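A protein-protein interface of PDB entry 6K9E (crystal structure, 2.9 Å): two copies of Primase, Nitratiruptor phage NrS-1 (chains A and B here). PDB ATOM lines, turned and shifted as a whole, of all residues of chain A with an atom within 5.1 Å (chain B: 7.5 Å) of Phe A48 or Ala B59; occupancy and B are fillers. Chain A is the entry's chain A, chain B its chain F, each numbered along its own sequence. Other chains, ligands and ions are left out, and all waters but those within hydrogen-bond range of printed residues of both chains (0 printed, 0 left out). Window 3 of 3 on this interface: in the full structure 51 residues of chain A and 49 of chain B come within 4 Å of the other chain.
No position is printed for both chains. Of the 13 pairs that touch across the chains among the printed residues, none has its exchanged pair printed and touching as well.
Among the printed residues, pairs that only touch across the chains: Phe A48 with Asn B57 (3.3 Å), Glu A49 with Pro B4 (3.6 Å), Phe A48 with Pro B4 (3.6 Å), Phe A48 with Glu B1 (3.6 Å), Phe A48 with Ala B59 (3.6 Å), Glu A49 with Pro B61 (3.7 Å), Glu A49 with Val B60 (3.7 Å), Gln A45 with Val B60 (3.8 Å) and Glu A49 with Leu B5 (3.9 Å).
The side-chain carboxylate (OD1) of Asp B3 lies close to the backbone NH (N) of Leu B5, 3.3 Å away. N of Tyr B8 sits at hydrogen-bond distance from O of Ala B59 (2.9 Å).
Of the 11 printed residues of chain A, 5 touch a printed residue of chain B. Hydrophobic or aromatic side chains of chain B within 4 Å of the printed part of chain A: Pro B4, Leu B5, Tyr B27, Ile B58, Ala B59 and Val B60. Among the printed residues, 13 pairs touch across the chains. Among the printed residues, no Asp or Glu carboxylate lies within 4 Å of a Lys or Arg side-chain nitrogen of the other chain.
Printed residues of chain A within 4 Å of Tyr B27: Gln A45. Leu B43 touches none of the printed residues of chain A. Ala B59 touches just one residue of chain A: Phe A48. Of the printed residues of chain A, Pro B61 touches Glu A49 (3.7 Å). The nearest residue of chain B that does not touch Phe A48 is Ile B58 (4.1 Å). The nearest residue of chain A that does not touch Ala B59 is Gln A45 (4.9 Å). The nearest printed residue of chain B that does not touch Thr A54 is Lys B56 (6.3 Å).
OG1 of Thr A54 lies within hydrogen-bond range of OD1 of Asn B57, at 2.9 Å. The side-chain amide oxygen of Gln A45 lies close to the side-chain hydroxyl of Tyr B27. NE2 of Gln A45 is in hydrogen-bond range of O of Ile B58, at 2.7 Å. The backbone NH (N) of Glu B1 is in hydrogen-bond range of the backbone carbonyl oxygen (O) of Gly A52 (3.2 Å).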
ATOM      1  N   GLN A  44       8.251  20.253  18.417  1.00  0.00           N
ATOM      2  CA  GLN A  44       7.404  21.029  17.517  1.00  0.00           C
ATOM      3  C   GLN A  44       6.059  21.359  18.150  1.00  0.00           C
ATOM      4  O   GLN A  44       5.503  22.430  17.893  1.00  0.00           O
ATOM      5  CB  GLN A  44       7.204  20.283  16.201  1.00  0.00           C
ATOM      6  CG  GLN A  44       8.479  19.921  15.472  1.00  0.00           C
ATOM      7  CD  GLN A  44       8.201  19.346  14.102  1.00  0.00           C
ATOM      8  OE1 GLN A  44       7.226  18.624  13.916  1.00  0.00           O
ATOM      9  NE2 GLN A  44       9.036  19.684  13.132  1.00  0.00           N
ATOM     10  N   GLN A  45       5.520  20.458  18.974  1.00  0.00           N
ATOM     11  CA  GLN A  45       4.282  20.764  19.682  1.00  0.00           C
ATOM     12  C   GLN A  45       4.480  21.867  20.706  1.00  0.00           C
ATOM     13  O   GLN A  45       3.560  22.652  20.960  1.00  0.00           O
ATOM     14  CB  GLN A  45       3.741  19.502  20.353  1.00  0.00           C
ATOM     15  CG  GLN A  45       2.613  19.751  21.325  1.00  0.00           C
ATOM     16  CD  GLN A  45       1.333  20.144  20.650  1.00  0.00           C
ATOM     17  OE1 GLN A  45       0.883  19.492  19.713  1.00  0.00           O
ATOM     18  NE2 GLN A  45       0.725  21.218  21.130  1.00  0.00           N
ATOM     19  N   ILE A  46       5.677  21.964  21.276  1.00  0.00           N
ATOM     20  CA  ILE A  46       5.951  23.012  22.247  1.00  0.00           C
ATOM     21  C   ILE A  46       6.047  24.366  21.566  1.00  0.00           C
ATOM     22  O   ILE A  46       5.494  25.355  22.054  1.00  0.00           O
ATOM     23  CB  ILE A  46       7.234  22.682  23.022  1.00  0.00           C
ATOM     24  CG1 ILE A  46       6.972  21.552  24.001  1.00  0.00           C
ATOM     25  CG2 ILE A  46       7.753  23.901  23.746  1.00  0.00           C
ATOM     26  CD1 ILE A  46       8.209  20.873  24.396  1.00  0.00           C
ATOM     27  N   VAL A  47       6.721  24.434  20.416  1.00  0.00           N
ATOM     28  CA  VAL A  47       6.978  25.740  19.819  1.00  0.00           C
ATOM     29  C   VAL A  47       5.725  26.295  19.166  1.00  0.00           C
ATOM     30  O   VAL A  47       5.553  27.515  19.087  1.00  0.00           O
ATOM     31  CB  VAL A  47       8.134  25.654  18.804  1.00  0.00           C
ATOM     32  CG1 VAL A  47       9.434  25.277  19.506  1.00  0.00           C
ATOM     33  CG2 VAL A  47       7.798  24.718  17.660  1.00  0.00           C
ATOM     34  N   PHE A  48       4.829  25.427  18.696  1.00  0.00           N
ATOM     35  CA  PHE A  48       3.552  25.909  18.186  1.00  0.00           C
ATOM     36  C   PHE A  48       2.770  26.650  19.259  1.00  0.00           C
ATOM     37  O   PHE A  48       2.141  27.675  18.982  1.00  0.00           O
ATOM     38  CB  PHE A  48       2.721  24.753  17.636  1.00  0.00           C
ATOM     39  CG  PHE A  48       1.350  25.163  17.185  1.00  0.00           C
ATOM     40  CD1 PHE A  48       1.146  25.659  15.909  1.00  0.00           C
ATOM     41  CD2 PHE A  48       0.263  25.059  18.038  1.00  0.00           C
ATOM     42  CE1 PHE A  48      -0.115  26.040  15.492  1.00  0.00           C
ATOM     43  CE2 PHE A  48      -0.999  25.440  17.626  1.00  0.00           C
ATOM     44  CZ  PHE A  48      -1.187  25.928  16.352  1.00  0.00           C
ATOM     45  N   GLU A  49       2.763  26.126  20.482  1.00  0.00           N
ATOM     46  CA  GLU A  49       2.037  26.802  21.549  1.00  0.00           C
ATOM     47  C   GLU A  49       2.693  28.129  21.920  1.00  0.00           C
ATOM     48  O   GLU A  49       2.004  29.057  22.359  1.00  0.00           O
ATOM     49  CB  GLU A  49       1.903  25.874  22.759  1.00  0.00           C
ATOM     50  CG  GLU A  49       1.176  26.480  23.945  1.00  0.00           C
ATOM     51  CD  GLU A  49       1.983  26.419  25.220  1.00  0.00           C
ATOM     52  OE1 GLU A  49       1.406  26.665  26.299  1.00  0.00           O
ATOM     53  OE2 GLU A  49       3.191  26.118  25.146  1.00  0.00           O
ATOM     54  N   ILE A  50       4.008  28.249  21.744  1.00  0.00           N
ATOM     55  CA  ILE A  50       4.706  29.472  22.137  1.00  0.00           C
ATOM     56  C   ILE A  50       4.751  30.502  21.012  1.00  0.00           C
ATOM     57  O   ILE A  50       4.570  31.696  21.260  1.00  0.00           O
ATOM     58  CB  ILE A  50       6.123  29.155  22.656  1.00  0.00           C
ATOM     59  CG1 ILE A  50       6.106  27.943  23.582  1.00  0.00           C
ATOM     60  CG2 ILE A  50       6.730  30.362  23.344  1.00  0.00           C
ATOM     61  CD1 ILE A  50       7.476  27.482  23.988  1.00  0.00           C
ATOM     62  N   ILE A  51       4.978  30.098  19.760  1.00  0.00           N
ATOM     63  CA  ILE A  51       5.163  31.076  18.696  1.00  0.00           C
ATOM     64  C   ILE A  51       4.113  30.950  17.599  1.00  0.00           C
ATOM     65  O   ILE A  51       4.185  31.658  16.598  1.00  0.00           O
ATOM     66  CB  ILE A  51       6.584  31.011  18.097  1.00  0.00           C
ATOM     67  CG1 ILE A  51       6.730  29.815  17.159  1.00  0.00           C
ATOM     68  CG2 ILE A  51       7.632  30.966  19.200  1.00  0.00           C
ATOM     69  CD1 ILE A  51       8.058  29.778  16.445  1.00  0.00           C
ATOM     70  N   GLY A  52       3.135  30.067  17.768  1.00  0.00           N
ATOM     71  CA  GLY A  52       1.992  30.019  16.878  1.00  0.00           C
ATOM     72  C   GLY A  52       2.184  29.376  15.522  1.00  0.00           C
ATOM     73  O   GLY A  52       1.273  29.466  14.692  1.00  0.00           O
ATOM     74  N   LYS A  53       3.323  28.744  15.253  1.00  0.00           N
ATOM     75  CA  LYS A  53       3.463  28.000  14.006  1.00  0.00           C
ATOM     76  C   LYS A  53       4.516  26.914  14.172  1.00  0.00           C
ATOM     77  O   LYS A  53       5.458  27.063  14.952  1.00  0.00           O
ATOM     78  CB  LYS A  53       3.819  28.921  12.835  1.00  0.00           C
ATOM     79  CG  LYS A  53       5.017  29.817  13.075  1.00  0.00           C
ATOM     80  CD  LYS A  53       5.373  30.579  11.810  1.00  0.00           C
ATOM     81  CE  LYS A  53       4.162  31.305  11.245  1.00  0.00           C
ATOM     82  NZ  LYS A  53       4.454  31.897   9.912  1.00  0.00           N
ATOM     83  N   THR A  54       4.346  25.820  13.422  1.00  0.00           N
ATOM     84  CA  THR A  54       5.263  24.692  13.483  1.00  0.00           C
ATOM     85  C   THR A  54       6.267  24.778  12.338  1.00  0.00           C
ATOM     86  O   THR A  54       5.922  24.461  11.189  1.00  0.00           O
ATOM     87  CB  THR A  54       4.497  23.367  13.429  1.00  0.00           C
ATOM     88  OG1 THR A  54       3.457  23.369  14.412  1.00  0.00           O
ATOM     89  CG2 THR A  54       5.437  22.204  13.703  1.00  0.00           C
ATOM     90  N   GLU B   1      -1.902  29.271  15.118  1.00  0.00           N
ATOM     91  CA  GLU B   1      -2.901  30.148  14.521  1.00  0.00           C
ATOM     92  C   GLU B   1      -2.948  31.490  15.245  1.00  0.00           C
ATOM     93  O   GLU B   1      -1.974  31.900  15.881  1.00  0.00           O
ATOM     94  CB  GLU B   1      -4.282  29.486  14.544  1.00  0.00           C
ATOM     95  N   LYS B   2      -4.092  32.172  15.138  1.00  0.00           N
ATOM     96  CA  LYS B   2      -4.264  33.448  15.826  1.00  0.00           C
ATOM     97  C   LYS B   2      -4.171  33.273  17.336  1.00  0.00           C
ATOM     98  O   LYS B   2      -3.679  34.158  18.044  1.00  0.00           O
ATOM     99  CB  LYS B   2      -5.605  34.071  15.439  1.00  0.00           C
ATOM    100  N   ASP B   3      -4.627  32.131  17.840  1.00  0.00           N
ATOM    101  CA  ASP B   3      -4.664  31.816  19.259  1.00  0.00           C
ATOM    102  C   ASP B   3      -4.208  30.374  19.447  1.00  0.00           C
ATOM    103  O   ASP B   3      -4.967  29.438  19.161  1.00  0.00           O
ATOM    104  CB  ASP B   3      -6.076  32.030  19.811  1.00  0.00           C
ATOM    105  CG  ASP B   3      -6.211  31.632  21.263  1.00  0.00           C
ATOM    106  OD1 ASP B   3      -5.181  31.527  21.962  1.00  0.00           O
ATOM    107  OD2 ASP B   3      -7.359  31.432  21.708  1.00  0.00           O
ATOM    108  N   PRO B   4      -2.992  30.149  19.939  1.00  0.00           N
ATOM    109  CA  PRO B   4      -2.445  28.786  19.956  1.00  0.00           C
ATOM    110  C   PRO B   4      -3.094  27.889  20.999  1.00  0.00           C
ATOM    111  O   PRO B   4      -2.626  26.772  21.236  1.00  0.00           O
ATOM    112  CB  PRO B   4      -0.952  29.005  20.244  1.00  0.00           C
ATOM    113  CG  PRO B   4      -0.802  30.462  20.634  1.00  0.00           C
ATOM    114  CD  PRO B   4      -2.161  31.085  20.707  1.00  0.00           C
ATOM    115  N   LEU B   5      -4.151  28.372  21.647  1.00  0.00           N
ATOM    116  CA  LEU B   5      -4.934  27.564  22.571  1.00  0.00           C
ATOM    117  C   LEU B   5      -6.405  27.556  22.176  1.00  0.00           C
ATOM    118  O   LEU B   5      -7.281  27.385  23.025  1.00  0.00           O
ATOM    119  CB  LEU B   5      -4.778  28.048  24.015  1.00  0.00           C
ATOM    120  CG  LEU B   5      -3.497  27.845  24.838  1.00  0.00           C
ATOM    121  CD1 LEU B   5      -2.233  28.334  24.153  1.00  0.00           C
ATOM    122  CD2 LEU B   5      -3.646  28.506  26.199  1.00  0.00           C
ATOM    123  N   TRP B   6      -6.691  27.724  20.883  1.00  0.00           N
ATOM    124  CA  TRP B   6      -8.081  27.731  20.440  1.00  0.00           C
ATOM    125  C   TRP B   6      -8.715  26.362  20.628  1.00  0.00           C
ATOM    126  O   TRP B   6      -9.848  26.255  21.106  1.00  0.00           O
ATOM    127  CB  TRP B   6      -8.179  28.171  18.976  1.00  0.00           C
ATOM    128  CG  TRP B   6      -7.759  27.135  17.967  1.00  0.00           C
ATOM    129  CD1 TRP B   6      -6.528  26.989  17.405  1.00  0.00           C
ATOM    130  CD2 TRP B   6      -8.582  26.107  17.397  1.00  0.00           C
ATOM    131  NE1 TRP B   6      -6.530  25.933  16.525  1.00  0.00           N
ATOM    132  CE2 TRP B   6      -7.780  25.375  16.504  1.00  0.00           C
ATOM    133  CE3 TRP B   6      -9.919  25.732  17.564  1.00  0.00           C
ATOM    134  CZ2 TRP B   6      -8.268  24.296  15.776  1.00  0.00           C
ATOM    135  CZ3 TRP B   6     -10.401  24.660  16.839  1.00  0.00           C
ATOM    136  CH2 TRP B   6      -9.578  23.954  15.958  1.00  0.00           C
ATOM    137  N   LEU B   7      -7.989  25.307  20.260  1.00  0.00           N
ATOM    138  CA  LEU B   7      -8.521  23.955  20.353  1.00  0.00           C
ATOM    139  C   LEU B   7      -8.750  23.582  21.808  1.00  0.00           C
ATOM    140  O   LEU B   7      -9.784  23.003  22.155  1.00  0.00           O
ATOM    141  CB  LEU B   7      -7.539  22.990  19.679  1.00  0.00           C
ATOM    142  CG  LEU B   7      -7.811  21.502  19.445  1.00  0.00           C
ATOM    143  CD1 LEU B   7      -7.527  20.641  20.666  1.00  0.00           C
ATOM    144  CD2 LEU B   7      -9.209  21.274  18.904  1.00  0.00           C
ATOM    145  N   TYR B   8      -7.811  23.960  22.679  1.00  0.00           N
ATOM    146  CA  TYR B   8      -7.929  23.691  24.110  1.00  0.00           C
ATOM    147  C   TYR B   8      -9.227  24.244  24.682  1.00  0.00           C
ATOM    148  O   TYR B   8      -9.902  23.575  25.471  1.00  0.00           O
ATOM    149  CB  TYR B   8      -6.726  24.300  24.836  1.00  0.00           C
ATOM    150  CG  TYR B   8      -6.740  24.245  26.354  1.00  0.00           C
ATOM    151  CD1 TYR B   8      -7.196  23.112  27.028  1.00  0.00           C
ATOM    152  CD2 TYR B   8      -6.268  25.328  27.113  1.00  0.00           C
ATOM    153  CE1 TYR B   8      -7.191  23.057  28.405  1.00  0.00           C
ATOM    154  CE2 TYR B   8      -6.262  25.280  28.495  1.00  0.00           C
ATOM    155  CZ  TYR B   8      -6.731  24.143  29.131  1.00  0.00           C
ATOM    156  OH  TYR B   8      -6.732  24.082  30.499  1.00  0.00           O
ATOM    157  N   LYS B   9      -9.590  25.469  24.294  1.00  0.00           N
ATOM    158  CA  LYS B   9     -10.764  26.113  24.874  1.00  0.00           C
ATOM    159  C   LYS B   9     -12.063  25.504  24.367  1.00  0.00           C
ATOM    160  O   LYS B   9     -12.988  25.264  25.151  1.00  0.00           O
ATOM    161  CB  LYS B   9     -10.737  27.605  24.560  1.00  0.00           C
ATOM    162  CG  LYS B   9      -9.525  28.328  25.084  1.00  0.00           C
ATOM    163  CD  LYS B   9      -9.508  29.754  24.582  1.00  0.00           C
ATOM    164  CE  LYS B   9      -8.205  30.424  24.935  1.00  0.00           C
ATOM    165  NZ  LYS B   9      -7.810  31.414  23.908  1.00  0.00           N
ATOM    166  N   VAL B  10     -12.143  25.223  23.065  1.00  0.00           N
ATOM    167  CA  VAL B  10     -13.395  24.725  22.508  1.00  0.00           C
ATOM    168  C   VAL B  10     -13.705  23.336  23.044  1.00  0.00           C
ATOM    169  O   VAL B  10     -14.874  22.949  23.126  1.00  0.00           O
ATOM    170  CB  VAL B  10     -13.377  24.751  20.967  1.00  0.00           C
ATOM    171  CG1 VAL B  10     -12.918  26.105  20.450  1.00  0.00           C
ATOM    172  CG2 VAL B  10     -12.514  23.637  20.422  1.00  0.00           C
ATOM    173  N   LEU B  11     -12.686  22.555  23.414  1.00  0.00           N
ATOM    174  CA  LEU B  11     -12.981  21.271  24.039  1.00  0.00           C
ATOM    175  C   LEU B  11     -13.382  21.426  25.496  1.00  0.00           C
ATOM    176  O   LEU B  11     -14.215  20.664  25.991  1.00  0.00           O
ATOM    177  CB  LEU B  11     -11.773  20.340  23.946  1.00  0.00           C
ATOM    178  CG  LEU B  11     -11.606  19.510  22.683  1.00  0.00           C
ATOM    179  CD1 LEU B  11     -10.910  20.297  21.646  1.00  0.00           C
ATOM    180  CD2 LEU B  11     -10.840  18.225  22.966  1.00  0.00           C
ATOM    181  N   VAL B  18      -7.606  18.633  27.586  1.00  0.00           N
ATOM    182  CA  VAL B  18      -6.430  17.973  27.030  1.00  0.00           C
ATOM    183  C   VAL B  18      -5.232  18.912  27.120  1.00  0.00           C
ATOM    184  O   VAL B  18      -5.361  20.123  26.916  1.00  0.00           O
ATOM    185  CB  VAL B  18      -6.666  17.494  25.581  1.00  0.00           C
ATOM    186  CG1 VAL B  18      -7.987  16.768  25.479  1.00  0.00           C
ATOM    187  CG2 VAL B  18      -6.640  18.638  24.609  1.00  0.00           C
ATOM    188  N   TYR B  27      -0.027  13.160  25.080  1.00  0.00           N
ATOM    189  CA  TYR B  27      -1.110  14.095  25.321  1.00  0.00           C
ATOM    190  C   TYR B  27      -2.006  13.535  26.408  1.00  0.00           C
ATOM    191  O   TYR B  27      -2.429  12.378  26.342  1.00  0.00           O
ATOM    192  CB  TYR B  27      -1.912  14.358  24.048  1.00  0.00           C
ATOM    193  CG  TYR B  27      -1.128  15.095  22.998  1.00  0.00           C
ATOM    194  CD1 TYR B  27      -0.218  14.432  22.192  1.00  0.00           C
ATOM    195  CD2 TYR B  27      -1.268  16.463  22.840  1.00  0.00           C
ATOM    196  CE1 TYR B  27       0.512  15.108  21.237  1.00  0.00           C
ATOM    197  CE2 TYR B  27      -0.541  17.147  21.890  1.00  0.00           C
ATOM    198  CZ  TYR B  27       0.348  16.464  21.092  1.00  0.00           C
ATOM    199  OH  TYR B  27       1.076  17.140  20.145  1.00  0.00           O
ATOM    200  N   LEU B  43      -5.369  11.339  19.799  1.00  0.00           N
ATOM    201  CA  LEU B  43      -6.097  12.543  20.178  1.00  0.00           C
ATOM    202  C   LEU B  43      -6.761  13.198  18.973  1.00  0.00           C
ATOM    203  O   LEU B  43      -7.832  13.800  19.107  1.00  0.00           O
ATOM    204  CB  LEU B  43      -5.151  13.521  20.869  1.00  0.00           C
ATOM    205  CG  LEU B  43      -5.581  14.981  20.979  1.00  0.00           C
ATOM    206  CD1 LEU B  43      -6.783  15.112  21.884  1.00  0.00           C
ATOM    207  CD2 LEU B  43      -4.439  15.816  21.494  1.00  0.00           C
ATOM    208  N   PRO B  55      -7.357  18.954  13.218  1.00  0.00           N
ATOM    209  CA  PRO B  55      -6.275  19.942  13.265  1.00  0.00           C
ATOM    210  C   PRO B  55      -4.968  19.295  12.839  1.00  0.00           C
ATOM    211  O   PRO B  55      -4.726  18.117  13.102  1.00  0.00           O
ATOM    212  CB  PRO B  55      -6.234  20.355  14.746  1.00  0.00           C
ATOM    213  CG  PRO B  55      -7.460  19.766  15.380  1.00  0.00           C
ATOM    214  CD  PRO B  55      -7.816  18.573  14.556  1.00  0.00           C
ATOM    215  N   LYS B  56      -4.124  20.061  12.154  1.00  0.00           N
ATOM    216  CA  LYS B  56      -2.779  19.559  11.923  1.00  0.00           C
ATOM    217  C   LYS B  56      -1.856  19.850  13.097  1.00  0.00           C
ATOM    218  O   LYS B  56      -0.965  19.043  13.394  1.00  0.00           O
ATOM    219  CB  LYS B  56      -2.182  20.136  10.635  1.00  0.00           C
ATOM    220  CG  LYS B  56      -0.805  19.549  10.337  1.00  0.00           C
ATOM    221  CD  LYS B  56      -0.250  19.922   8.974  1.00  0.00           C
ATOM    222  CE  LYS B  56       1.152  19.326   8.796  1.00  0.00           C
ATOM    223  NZ  LYS B  56       1.688  19.466   7.409  1.00  0.00           N
ATOM    224  N   ASN B  57      -2.061  20.974  13.779  1.00  0.00           N
ATOM    225  CA  ASN B  57      -1.308  21.335  14.974  1.00  0.00           C
ATOM    226  C   ASN B  57      -2.258  21.384  16.160  1.00  0.00           C
ATOM    227  O   ASN B  57      -3.333  21.987  16.075  1.00  0.00           O
ATOM    228  CB  ASN B  57      -0.593  22.679  14.795  1.00  0.00           C
ATOM    229  CG  ASN B  57       0.398  22.674  13.632  1.00  0.00           C
ATOM    230  OD1 ASN B  57       0.873  23.726  13.204  1.00  0.00           O
ATOM    231  ND2 ASN B  57       0.726  21.483  13.131  1.00  0.00           N
ATOM    232  N   ILE B  58      -1.873  20.739  17.255  1.00  0.00           N
ATOM    233  CA  ILE B  58      -2.752  20.573  18.403  1.00  0.00           C
ATOM    234  C   ILE B  58      -2.596  21.819  19.268  1.00  0.00           C
ATOM    235  O   ILE B  58      -1.628  21.951  20.015  1.00  0.00           O
ATOM    236  CB  ILE B  58      -2.424  19.301  19.180  1.00  0.00           C
ATOM    237  CG1 ILE B  58      -2.135  18.148  18.220  1.00  0.00           C
ATOM    238  CG2 ILE B  58      -3.584  18.945  20.108  1.00  0.00           C
ATOM    239  CD1 ILE B  58      -3.330  17.660  17.470  1.00  0.00           C
ATOM    240  N   ALA B  59      -3.543  22.748  19.147  1.00  0.00           N
ATOM    241  CA  ALA B  59      -3.476  24.013  19.872  1.00  0.00           C
ATOM    242  C   ALA B  59      -3.900  23.769  21.317  1.00  0.00           C
ATOM    243  O   ALA B  59      -5.019  24.068  21.737  1.00  0.00           O
ATOM    244  CB  ALA B  59      -4.346  25.064  19.200  1.00  0.00           C
ATOM    245  N   VAL B  60      -2.973  23.212  22.092  1.00  0.00           N
ATOM    246  CA  VAL B  60      -3.208  22.869  23.495  1.00  0.00           C
ATOM    247  C   VAL B  60      -2.008  23.286  24.316  1.00  0.00           C
ATOM    248  O   VAL B  60      -0.881  23.407  23.792  1.00  0.00           O
ATOM    249  CB  VAL B  60      -3.479  21.360  23.678  1.00  0.00           C
ATOM    250  CG1 VAL B  60      -4.669  20.934  22.850  1.00  0.00           C
ATOM    251  CG2 VAL B  60      -2.260  20.557  23.306  1.00  0.00           C
ATOM    252  N   PRO B  61      -2.193  23.528  25.613  1.00  0.00           N
ATOM    253  CA  PRO B  61      -1.083  23.976  26.454  1.00  0.00           C
ATOM    254  C   PRO B  61      -0.119  22.838  26.747  1.00  0.00           C
ATOM    255  O   PRO B  61      -0.376  21.669  26.456  1.00  0.00           O
ATOM    256  CB  PRO B  61      -1.757  24.471  27.735  1.00  0.00           C
ATOM    257  CG  PRO B  61      -3.089  23.849  27.754  1.00  0.00           C
ATOM    258  CD  PRO B  61      -3.445  23.374  26.381  1.00  0.00           C
